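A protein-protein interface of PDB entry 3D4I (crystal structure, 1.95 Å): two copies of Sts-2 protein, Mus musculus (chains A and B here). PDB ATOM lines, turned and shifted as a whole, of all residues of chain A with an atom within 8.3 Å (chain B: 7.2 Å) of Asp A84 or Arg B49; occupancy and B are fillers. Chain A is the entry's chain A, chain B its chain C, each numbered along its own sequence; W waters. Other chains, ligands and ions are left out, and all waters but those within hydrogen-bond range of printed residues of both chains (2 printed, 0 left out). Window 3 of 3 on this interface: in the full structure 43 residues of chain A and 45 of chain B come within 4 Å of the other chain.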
ATOM      1  N   LEU A  77      -8.732  -2.245 -15.963  1.00  0.00           N
ATOM      2  CA  LEU A  77     -10.049  -1.595 -15.933  1.00  0.00           C
ATOM      3  C   LEU A  77     -11.160  -2.586 -15.563  1.00  0.00           C
ATOM      4  O   LEU A  77     -12.036  -2.292 -14.731  1.00  0.00           O
ATOM      5  CB  LEU A  77     -10.361  -0.932 -17.289  1.00  0.00           C
ATOM      6  CG  LEU A  77     -11.490   0.112 -17.329  1.00  0.00           C
ATOM      7  CD1 LEU A  77     -11.043   1.397 -16.594  1.00  0.00           C
ATOM      8  CD2 LEU A  77     -11.844   0.397 -18.760  1.00  0.00           C
ATOM      9  N   ALA A  78     -11.130  -3.751 -16.190  1.00  0.00           N
ATOM     10  CA  ALA A  78     -12.010  -4.876 -15.809  1.00  0.00           C
ATOM     11  C   ALA A  78     -11.872  -5.307 -14.335  1.00  0.00           C
ATOM     12  O   ALA A  78     -12.880  -5.518 -13.662  1.00  0.00           O
ATOM     13  CB  ALA A  78     -11.756  -6.073 -16.736  1.00  0.00           C
ATOM     14  N   GLY A  79     -10.646  -5.466 -13.847  1.00  0.00           N
ATOM     15  CA  GLY A  79     -10.406  -5.825 -12.435  1.00  0.00           C
ATOM     16  C   GLY A  79     -10.980  -4.783 -11.472  1.00  0.00           C
ATOM     17  O   GLY A  79     -11.619  -5.117 -10.470  1.00  0.00           O
ATOM     18  N   GLU A  80     -10.738  -3.515 -11.777  1.00  0.00           N
ATOM     19  CA  GLU A  80     -11.309  -2.392 -11.026  1.00  0.00           C
ATOM     20  C   GLU A  80     -12.843  -2.397 -11.019  1.00  0.00           C
ATOM     21  O   GLU A  80     -13.466  -2.169  -9.958  1.00  0.00           O
ATOM     22  CB  GLU A  80     -10.763  -1.066 -11.557  1.00  0.00           C
ATOM     23  CG  GLU A  80     -11.287   0.161 -10.780  1.00  0.00           C
ATOM     24  CD  GLU A  80     -10.928   1.446 -11.497  1.00  0.00           C
ATOM     25  OE1 GLU A  80     -11.092   1.504 -12.729  1.00  0.00           O
ATOM     26  OE2 GLU A  80     -10.474   2.381 -10.831  1.00  0.00           O
ATOM     27  N   ALA A  81     -13.458  -2.683 -12.169  1.00  0.00           N
ATOM     28  CA  ALA A  81     -14.925  -2.809 -12.234  1.00  0.00           C
ATOM     29  C   ALA A  81     -15.411  -3.982 -11.379  1.00  0.00           C
ATOM     30  O   ALA A  81     -16.413  -3.867 -10.660  1.00  0.00           O
ATOM     31  CB  ALA A  81     -15.409  -2.961 -13.681  1.00  0.00           C
ATOM     32  N   LEU A  82     -14.698  -5.109 -11.447  1.00  0.00           N
ATOM     33  CA  LEU A  82     -15.006  -6.240 -10.581  1.00  0.00           C
ATOM     34  C   LEU A  82     -14.948  -5.859  -9.114  1.00  0.00           C
ATOM     35  O   LEU A  82     -15.864  -6.212  -8.361  1.00  0.00           O
ATOM     36  CB  LEU A  82     -14.103  -7.448 -10.867  1.00  0.00           C
ATOM     37  CG  LEU A  82     -14.509  -8.209 -12.132  1.00  0.00           C
ATOM     38  CD1 LEU A  82     -13.363  -9.088 -12.646  1.00  0.00           C
ATOM     39  CD2 LEU A  82     -15.832  -9.050 -11.894  1.00  0.00           C
ATOM     40  N   LEU A  83     -13.899  -5.149  -8.704  1.00  0.00           N
ATOM     41  CA  LEU A  83     -13.854  -4.607  -7.331  1.00  0.00           C
ATOM     42  C   LEU A  83     -15.094  -3.762  -7.009  1.00  0.00           C
ATOM     43  O   LEU A  83     -15.747  -3.981  -5.975  1.00  0.00           O
ATOM     44  CB  LEU A  83     -12.561  -3.804  -7.045  1.00  0.00           C
ATOM     45  CG  LEU A  83     -12.358  -3.382  -5.579  1.00  0.00           C
ATOM     46  CD1 LEU A  83     -12.261  -4.625  -4.676  1.00  0.00           C
ATOM     47  CD2 LEU A  83     -11.129  -2.493  -5.402  1.00  0.00           C
ATOM     48  N   ASP A  84     -15.405  -2.810  -7.895  1.00  0.00           N
ATOM     49  CA  ASP A  84     -16.543  -1.898  -7.721  1.00  0.00           C
ATOM     50  C   ASP A  84     -17.877  -2.644  -7.573  1.00  0.00           C
ATOM     51  O   ASP A  84     -18.765  -2.238  -6.803  1.00  0.00           O
ATOM     52  CB  ASP A  84     -16.613  -0.922  -8.908  1.00  0.00           C
ATOM     53  CG  ASP A  84     -15.483   0.124  -8.898  1.00  0.00           C
ATOM     54  OD1 ASP A  84     -14.702   0.209  -7.917  1.00  0.00           O
ATOM     55  OD2 ASP A  84     -15.376   0.860  -9.905  1.00  0.00           O
ATOM     56  N   SER A  85     -18.010  -3.754  -8.293  1.00  0.00           N
ATOM     57  CA  SER A  85     -19.248  -4.534  -8.286  1.00  0.00           C
ATOM     58  C   SER A  85     -19.552  -5.257  -6.961  1.00  0.00           C
ATOM     59  O   SER A  85     -20.685  -5.699  -6.742  1.00  0.00           O
ATOM     60  CB  SER A  85     -19.238  -5.546  -9.422  1.00  0.00           C
ATOM     61  OG  SER A  85     -18.444  -6.663  -9.066  1.00  0.00           O
ATOM     62  N   GLY A  86     -18.547  -5.411  -6.113  1.00  0.00           N
ATOM     63  CA  GLY A  86     -18.715  -6.081  -4.833  1.00  0.00           C
ATOM     64  C   GLY A  86     -18.772  -7.606  -4.862  1.00  0.00           C
ATOM     65  O   GLY A  86     -18.915  -8.237  -3.817  1.00  0.00           O
ATOM     66  N   VAL A  87     -18.675  -8.215  -6.039  1.00  0.00           N
ATOM     67  CA  VAL A  87     -18.733  -9.675  -6.126  1.00  0.00           C
ATOM     68  C   VAL A  87     -17.544 -10.347  -5.417  1.00  0.00           C
ATOM     69  O   VAL A  87     -16.453  -9.778  -5.315  1.00  0.00           O
ATOM     70  CB  VAL A  87     -18.876 -10.202  -7.598  1.00  0.00           C
ATOM     71  CG1 VAL A  87     -20.075  -9.579  -8.257  1.00  0.00           C
ATOM     72  CG2 VAL A  87     -17.587  -9.974  -8.424  1.00  0.00           C
ATOM     73  N   GLU A 110      -5.944  -5.368  -9.311  1.00  0.00           N
ATOM     74  CA  GLU A 110      -6.993  -4.360  -9.145  1.00  0.00           C
ATOM     75  C   GLU A 110      -8.108  -4.799  -8.210  1.00  0.00           C
ATOM     76  O   GLU A 110      -8.783  -3.958  -7.610  1.00  0.00           O
ATOM     77  CB  GLU A 110      -7.583  -3.953 -10.486  1.00  0.00           C
ATOM     78  CG  GLU A 110      -6.636  -3.151 -11.373  1.00  0.00           C
ATOM     79  CD  GLU A 110      -6.234  -1.823 -10.785  1.00  0.00           C
ATOM     80  OE1 GLU A 110      -7.068  -1.158 -10.104  1.00  0.00           O
ATOM     81  OE2 GLU A 110      -5.059  -1.461 -10.990  1.00  0.00           O
ATOM     82  N   LEU A 111      -8.303  -6.113  -8.095  1.00  0.00           N
ATOM     83  CA  LEU A 111      -9.209  -6.672  -7.083  1.00  0.00           C
ATOM     84  C   LEU A 111      -8.614  -6.653  -5.671  1.00  0.00           C
ATOM     85  O   LEU A 111      -9.323  -6.917  -4.707  1.00  0.00           O
ATOM     86  CB  LEU A 111      -9.520  -8.133  -7.417  1.00  0.00           C
ATOM     87  CG  LEU A 111     -10.866  -8.748  -7.822  1.00  0.00           C
ATOM     88  CD1 LEU A 111     -12.133  -7.912  -7.499  1.00  0.00           C
ATOM     89  CD2 LEU A 111     -10.875  -9.270  -9.219  1.00  0.00           C
ATOM     90  N   PRO A 254     -21.163  -9.687 -14.311  1.00  0.00           N
ATOM     91  CA  PRO A 254     -21.283  -8.735 -13.200  1.00  0.00           C
ATOM     92  C   PRO A 254     -20.693  -7.351 -13.501  1.00  0.00           C
ATOM     93  O   PRO A 254     -20.826  -6.445 -12.697  1.00  0.00           O
ATOM     94  CB  PRO A 254     -20.459  -9.397 -12.089  1.00  0.00           C
ATOM     95  CG  PRO A 254     -19.439 -10.201 -12.814  1.00  0.00           C
ATOM     96  CD  PRO A 254     -20.194 -10.760 -14.000  1.00  0.00           C
ATOM     97  N   VAL A 255     -20.015  -7.214 -14.633  1.00  0.00           N
ATOM     98  CA  VAL A 255     -19.445  -5.918 -15.020  1.00  0.00           C
ATOM     99  C   VAL A 255     -19.747  -5.634 -16.480  1.00  0.00           C
ATOM    100  O   VAL A 255     -19.992  -6.558 -17.255  1.00  0.00           O
ATOM    101  CB  VAL A 255     -17.918  -5.807 -14.724  1.00  0.00           C
ATOM    102  CG1 VAL A 255     -17.660  -5.839 -13.238  1.00  0.00           C
ATOM    103  CG2 VAL A 255     -17.125  -6.874 -15.414  1.00  0.00           C
ATOM    104  N   TYR B  40     -25.530   9.656 -12.104  1.00  0.00           N
ATOM    105  CA  TYR B  40     -24.534   9.098 -13.013  1.00  0.00           C
ATOM    106  C   TYR B  40     -24.402   7.591 -12.831  1.00  0.00           C
ATOM    107  O   TYR B  40     -24.366   7.078 -11.703  1.00  0.00           O
ATOM    108  CB  TYR B  40     -23.174   9.794 -12.837  1.00  0.00           C
ATOM    109  CG  TYR B  40     -22.113   9.339 -13.819  1.00  0.00           C
ATOM    110  CD1 TYR B  40     -22.146   9.730 -15.150  1.00  0.00           C
ATOM    111  CD2 TYR B  40     -21.079   8.500 -13.410  1.00  0.00           C
ATOM    112  CE1 TYR B  40     -21.151   9.296 -16.053  1.00  0.00           C
ATOM    113  CE2 TYR B  40     -20.092   8.065 -14.301  1.00  0.00           C
ATOM    114  CZ  TYR B  40     -20.137   8.464 -15.610  1.00  0.00           C
ATOM    115  OH  TYR B  40     -19.161   8.029 -16.474  1.00  0.00           O
ATOM    116  N   TYR B  41     -24.349   6.879 -13.954  1.00  0.00           N
ATOM    117  CA  TYR B  41     -23.966   5.477 -13.954  1.00  0.00           C
ATOM    118  C   TYR B  41     -23.123   5.179 -15.181  1.00  0.00           C
ATOM    119  O   TYR B  41     -23.143   5.924 -16.151  1.00  0.00           O
ATOM    120  CB  TYR B  41     -25.190   4.561 -13.937  1.00  0.00           C
ATOM    121  CG  TYR B  41     -26.080   4.661 -15.135  1.00  0.00           C
ATOM    122  CD1 TYR B  41     -27.019   5.677 -15.234  1.00  0.00           C
ATOM    123  CD2 TYR B  41     -26.032   3.699 -16.166  1.00  0.00           C
ATOM    124  CE1 TYR B  41     -27.873   5.755 -16.325  1.00  0.00           C
ATOM    125  CE2 TYR B  41     -26.873   3.789 -17.270  1.00  0.00           C
ATOM    126  CZ  TYR B  41     -27.793   4.822 -17.328  1.00  0.00           C
ATOM    127  OH  TYR B  41     -28.657   4.953 -18.389  1.00  0.00           O
ATOM    128  N   ARG B  42     -22.411   4.066 -15.123  1.00  0.00           N
ATOM    129  CA  ARG B  42     -21.439   3.693 -16.125  1.00  0.00           C
ATOM    130  C   ARG B  42     -21.989   2.513 -16.936  1.00  0.00           C
ATOM    131  O   ARG B  42     -21.903   1.378 -16.467  1.00  0.00           O
ATOM    132  CB  ARG B  42     -20.191   3.257 -15.351  1.00  0.00           C
ATOM    133  CG  ARG B  42     -18.887   3.494 -15.979  1.00  0.00           C
ATOM    134  CD  ARG B  42     -17.791   3.173 -14.945  1.00  0.00           C
ATOM    135  NE  ARG B  42     -16.518   2.933 -15.607  1.00  0.00           N
ATOM    136  CZ  ARG B  42     -15.566   2.128 -15.162  1.00  0.00           C
ATOM    137  NH1 ARG B  42     -15.710   1.436 -14.028  1.00  0.00           N
ATOM    138  NH2 ARG B  42     -14.477   1.977 -15.884  1.00  0.00           N
ATOM    139  N   LEU B  45     -17.561   0.267 -19.567  1.00  0.00           N
ATOM    140  CA  LEU B  45     -16.345   0.612 -18.798  1.00  0.00           C
ATOM    141  C   LEU B  45     -15.538   1.808 -19.361  1.00  0.00           C
ATOM    142  O   LEU B  45     -14.719   2.422 -18.655  1.00  0.00           O
ATOM    143  CB  LEU B  45     -15.458  -0.613 -18.583  1.00  0.00           C
ATOM    144  CG  LEU B  45     -16.113  -1.780 -17.822  1.00  0.00           C
ATOM    145  CD1 LEU B  45     -15.041  -2.809 -17.516  1.00  0.00           C
ATOM    146  CD2 LEU B  45     -16.759  -1.286 -16.505  1.00  0.00           C
ATOM    147  N   ASN B  46     -15.805   2.176 -20.602  1.00  0.00           N
ATOM    148  CA  ASN B  46     -15.107   3.328 -21.182  1.00  0.00           C
ATOM    149  C   ASN B  46     -15.653   4.687 -20.741  1.00  0.00           C
ATOM    150  O   ASN B  46     -15.023   5.733 -20.994  1.00  0.00           O
ATOM    151  CB  ASN B  46     -15.030   3.246 -22.710  1.00  0.00           C
ATOM    152  CG  ASN B  46     -13.833   4.006 -23.257  1.00  0.00           C
ATOM    153  OD1 ASN B  46     -12.802   4.098 -22.597  1.00  0.00           O
ATOM    154  ND2 ASN B  46     -13.969   4.564 -24.454  1.00  0.00           N
ATOM    155  N   PHE B  47     -16.806   4.673 -20.079  1.00  0.00           N
ATOM    156  CA  PHE B  47     -17.290   5.850 -19.384  1.00  0.00           C
ATOM    157  C   PHE B  47     -16.489   5.925 -18.089  1.00  0.00           C
ATOM    158  O   PHE B  47     -16.189   4.896 -17.486  1.00  0.00           O
ATOM    159  CB  PHE B  47     -18.788   5.734 -19.036  1.00  0.00           C
ATOM    160  CG  PHE B  47     -19.720   5.954 -20.209  1.00  0.00           C
ATOM    161  CD1 PHE B  47     -19.890   4.971 -21.179  1.00  0.00           C
ATOM    162  CD2 PHE B  47     -20.468   7.124 -20.301  1.00  0.00           C
ATOM    163  CE1 PHE B  47     -20.797   5.149 -22.238  1.00  0.00           C
ATOM    164  CE2 PHE B  47     -21.346   7.332 -21.356  1.00  0.00           C
ATOM    165  CZ  PHE B  47     -21.518   6.337 -22.332  1.00  0.00           C
ATOM    166  N   PRO B  48     -16.118   7.130 -17.670  1.00  0.00           N
ATOM    167  CA  PRO B  48     -15.317   7.305 -16.448  1.00  0.00           C
ATOM    168  C   PRO B  48     -16.084   6.906 -15.176  1.00  0.00           C
ATOM    169  O   PRO B  48     -17.298   6.815 -15.209  1.00  0.00           O
ATOM    170  CB  PRO B  48     -14.983   8.802 -16.466  1.00  0.00           C
ATOM    171  CG  PRO B  48     -16.047   9.433 -17.295  1.00  0.00           C
ATOM    172  CD  PRO B  48     -16.380   8.409 -18.357  1.00  0.00           C
ATOM    173  N   ARG B  49     -15.382   6.639 -14.077  1.00  0.00           N
ATOM    174  CA  ARG B  49     -16.039   6.159 -12.851  1.00  0.00           C
ATOM    175  C   ARG B  49     -16.846   7.243 -12.158  1.00  0.00           C
ATOM    176  O   ARG B  49     -17.700   6.940 -11.334  1.00  0.00           O
ATOM    177  CB  ARG B  49     -15.022   5.560 -11.854  1.00  0.00           C
ATOM    178  CG  ARG B  49     -14.460   4.208 -12.250  1.00  0.00           C
ATOM    179  CD  ARG B  49     -14.083   3.371 -11.034  1.00  0.00           C
ATOM    180  NE  ARG B  49     -13.183   4.092 -10.138  1.00  0.00           N
ATOM    181  CZ  ARG B  49     -13.169   3.951  -8.819  1.00  0.00           C
ATOM    182  NH1 ARG B  49     -14.014   3.124  -8.224  1.00  0.00           N
ATOM    183  NH2 ARG B  49     -12.309   4.654  -8.094  1.00  0.00           N
ATOM    184  N   SER B  50     -16.566   8.508 -12.476  1.00  0.00           N
ATOM    185  CA  SER B  50     -17.367   9.614 -11.974  1.00  0.00           C
ATOM    186  C   SER B  50     -17.226  10.809 -12.896  1.00  0.00           C
ATOM    187  O   SER B  50     -16.327  10.843 -13.718  1.00  0.00           O
ATOM    188  CB  SER B  50     -16.940  10.005 -10.541  1.00  0.00           C
ATOM    189  OG  SER B  50     -15.654  10.607 -10.557  1.00  0.00           O
ATOM    190  N   LEU B  51     -18.135  11.774 -12.764  1.00  0.00           N
ATOM    191  CA  LEU B  51     -18.016  13.063 -13.445  1.00  0.00           C
ATOM    192  C   LEU B  51     -17.728  14.125 -12.382  1.00  0.00           C
ATOM    193  O   LEU B  51     -18.254  14.007 -11.267  1.00  0.00           O
ATOM    194  CB  LEU B  51     -19.323  13.412 -14.168  1.00  0.00           C
ATOM    195  CG  LEU B  51     -19.742  12.577 -15.387  1.00  0.00           C
ATOM    196  CD1 LEU B  51     -21.092  13.059 -15.911  1.00  0.00           C
ATOM    197  CD2 LEU B  51     -18.694  12.605 -16.507  1.00  0.00           C
ATOM    198  N   SER B  69     -12.307   6.386 -20.332  1.00  0.00           N
ATOM    199  CA  SER B  69     -11.291   5.583 -19.645  1.00  0.00           C
ATOM    200  C   SER B  69     -10.026   5.340 -20.481  1.00  0.00           C
ATOM    201  O   SER B  69      -8.906   5.398 -19.965  1.00  0.00           O
ATOM    202  CB  SER B  69     -11.894   4.245 -19.210  1.00  0.00           C
ATOM    203  OG  SER B  69     -12.915   4.525 -18.270  1.00  0.00           O
ATOM    204  N   ILE B  72      -7.918   8.397 -20.595  1.00  0.00           N
ATOM    205  CA  ILE B  72      -7.133   8.521 -19.352  1.00  0.00           C
ATOM    206  C   ILE B  72      -5.906   7.611 -19.434  1.00  0.00           C
ATOM    207  O   ILE B  72      -4.810   8.010 -19.061  1.00  0.00           O
ATOM    208  CB  ILE B  72      -7.979   8.206 -18.084  1.00  0.00           C
ATOM    209  CG1 ILE B  72      -9.050   9.288 -17.871  1.00  0.00           C
ATOM    210  CG2 ILE B  72      -7.057   8.060 -16.830  1.00  0.00           C
ATOM    211  CD1 ILE B  72     -10.275   8.790 -17.058  1.00  0.00           C
HETATM  212  O   HOH W   1     -13.058   0.258 -14.026  1.00  0.00           O
HETATM  213  O   HOH W   2     -17.382   0.823 -11.894  1.00  0.00           O
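Printed residues of chain B within 4 Å of Leu A77: Arg B42 (3.6 Å), Leu B45 (3.5 Å) and Ser B69 (3.9 Å). Of the printed residues of chain B, Ala A81 touches Leu B45. Of the printed residues of chain B, Asp A84 touches Arg B49 (3.0 Å). Of the printed residues of chain A, Arg B42 touches Leu A77 (3.6 Å). Phe B47 touches none of the printed residues of chain A. Arg B49 touches just these residues of chain A: Glu A80 and Asp A84. Ile B72 touches none of the printed residues of chain A. The nearest printed residue of chain B that does not touch Leu A77 is Asn B46 (4.7 Å).
Of the 12 printed residues of chain B, 4 touch a printed residue of chain A. Of the 15 printed residues of chain A, 4 touch a printed residue of chain B. Printed residues of chain A that touch a printed residue of chain B: Leu A77, Glu A80, Ala A81 and Asp A84. Among the printed residues, 6 pairs touch across the chains.
Water W1 lies within hydrogen-bond range of the side-chain carboxylate (OE1) of Glu A80, the backbone carbonyl oxygen (O) of Leu A77 and the guanidinium group (NH1) of Arg B42. Water W2 bridges NH1 of Arg B42 (2.8 Å) and OD2 of Asp A84 (2.8 Å).
No position is printed for both chains. Of the 6 pairs that touch across the chains among the printed residues, none has its exchanged pair printed and touching as well.
OE2 of Glu A80 is in salt-bridge range of NE of Arg B49, at 3.3 Å. OD1 of Asp A84 lies within salt-bridge range of NH1 of Arg B49 (3.0 Å).
O of Leu B45 lies within hydrogen-bond range of NH2 of Arg B42. NE of Arg B42 lies within hydrogen-bond range of O of Phe B47, 2.7 Å away. The backbone carbonyl oxygen (O) of Leu B45 sits at hydrogen-bond distance from the side-chain hydroxyl (OG) of Ser B69, at 2.8 Å. The backbone NH (N) of Ser B69 sits at hydrogen-bond distance from the backbone carbonyl oxygen (O) of Asn B46 (2.9 Å). The backbone carbonyl oxygen (O) of Phe B47 sits at hydrogen-bond distance from the side-chain hydroxyl (OG) of Ser B69.
Leu A77 touches Arg B42. Leu B45 touches Leu A77 (O to CD2, 3.5 Å). Ser B69 touches Leu A77. Ala A81 touches Leu B45 (CB to CD2, 3.6 Å).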
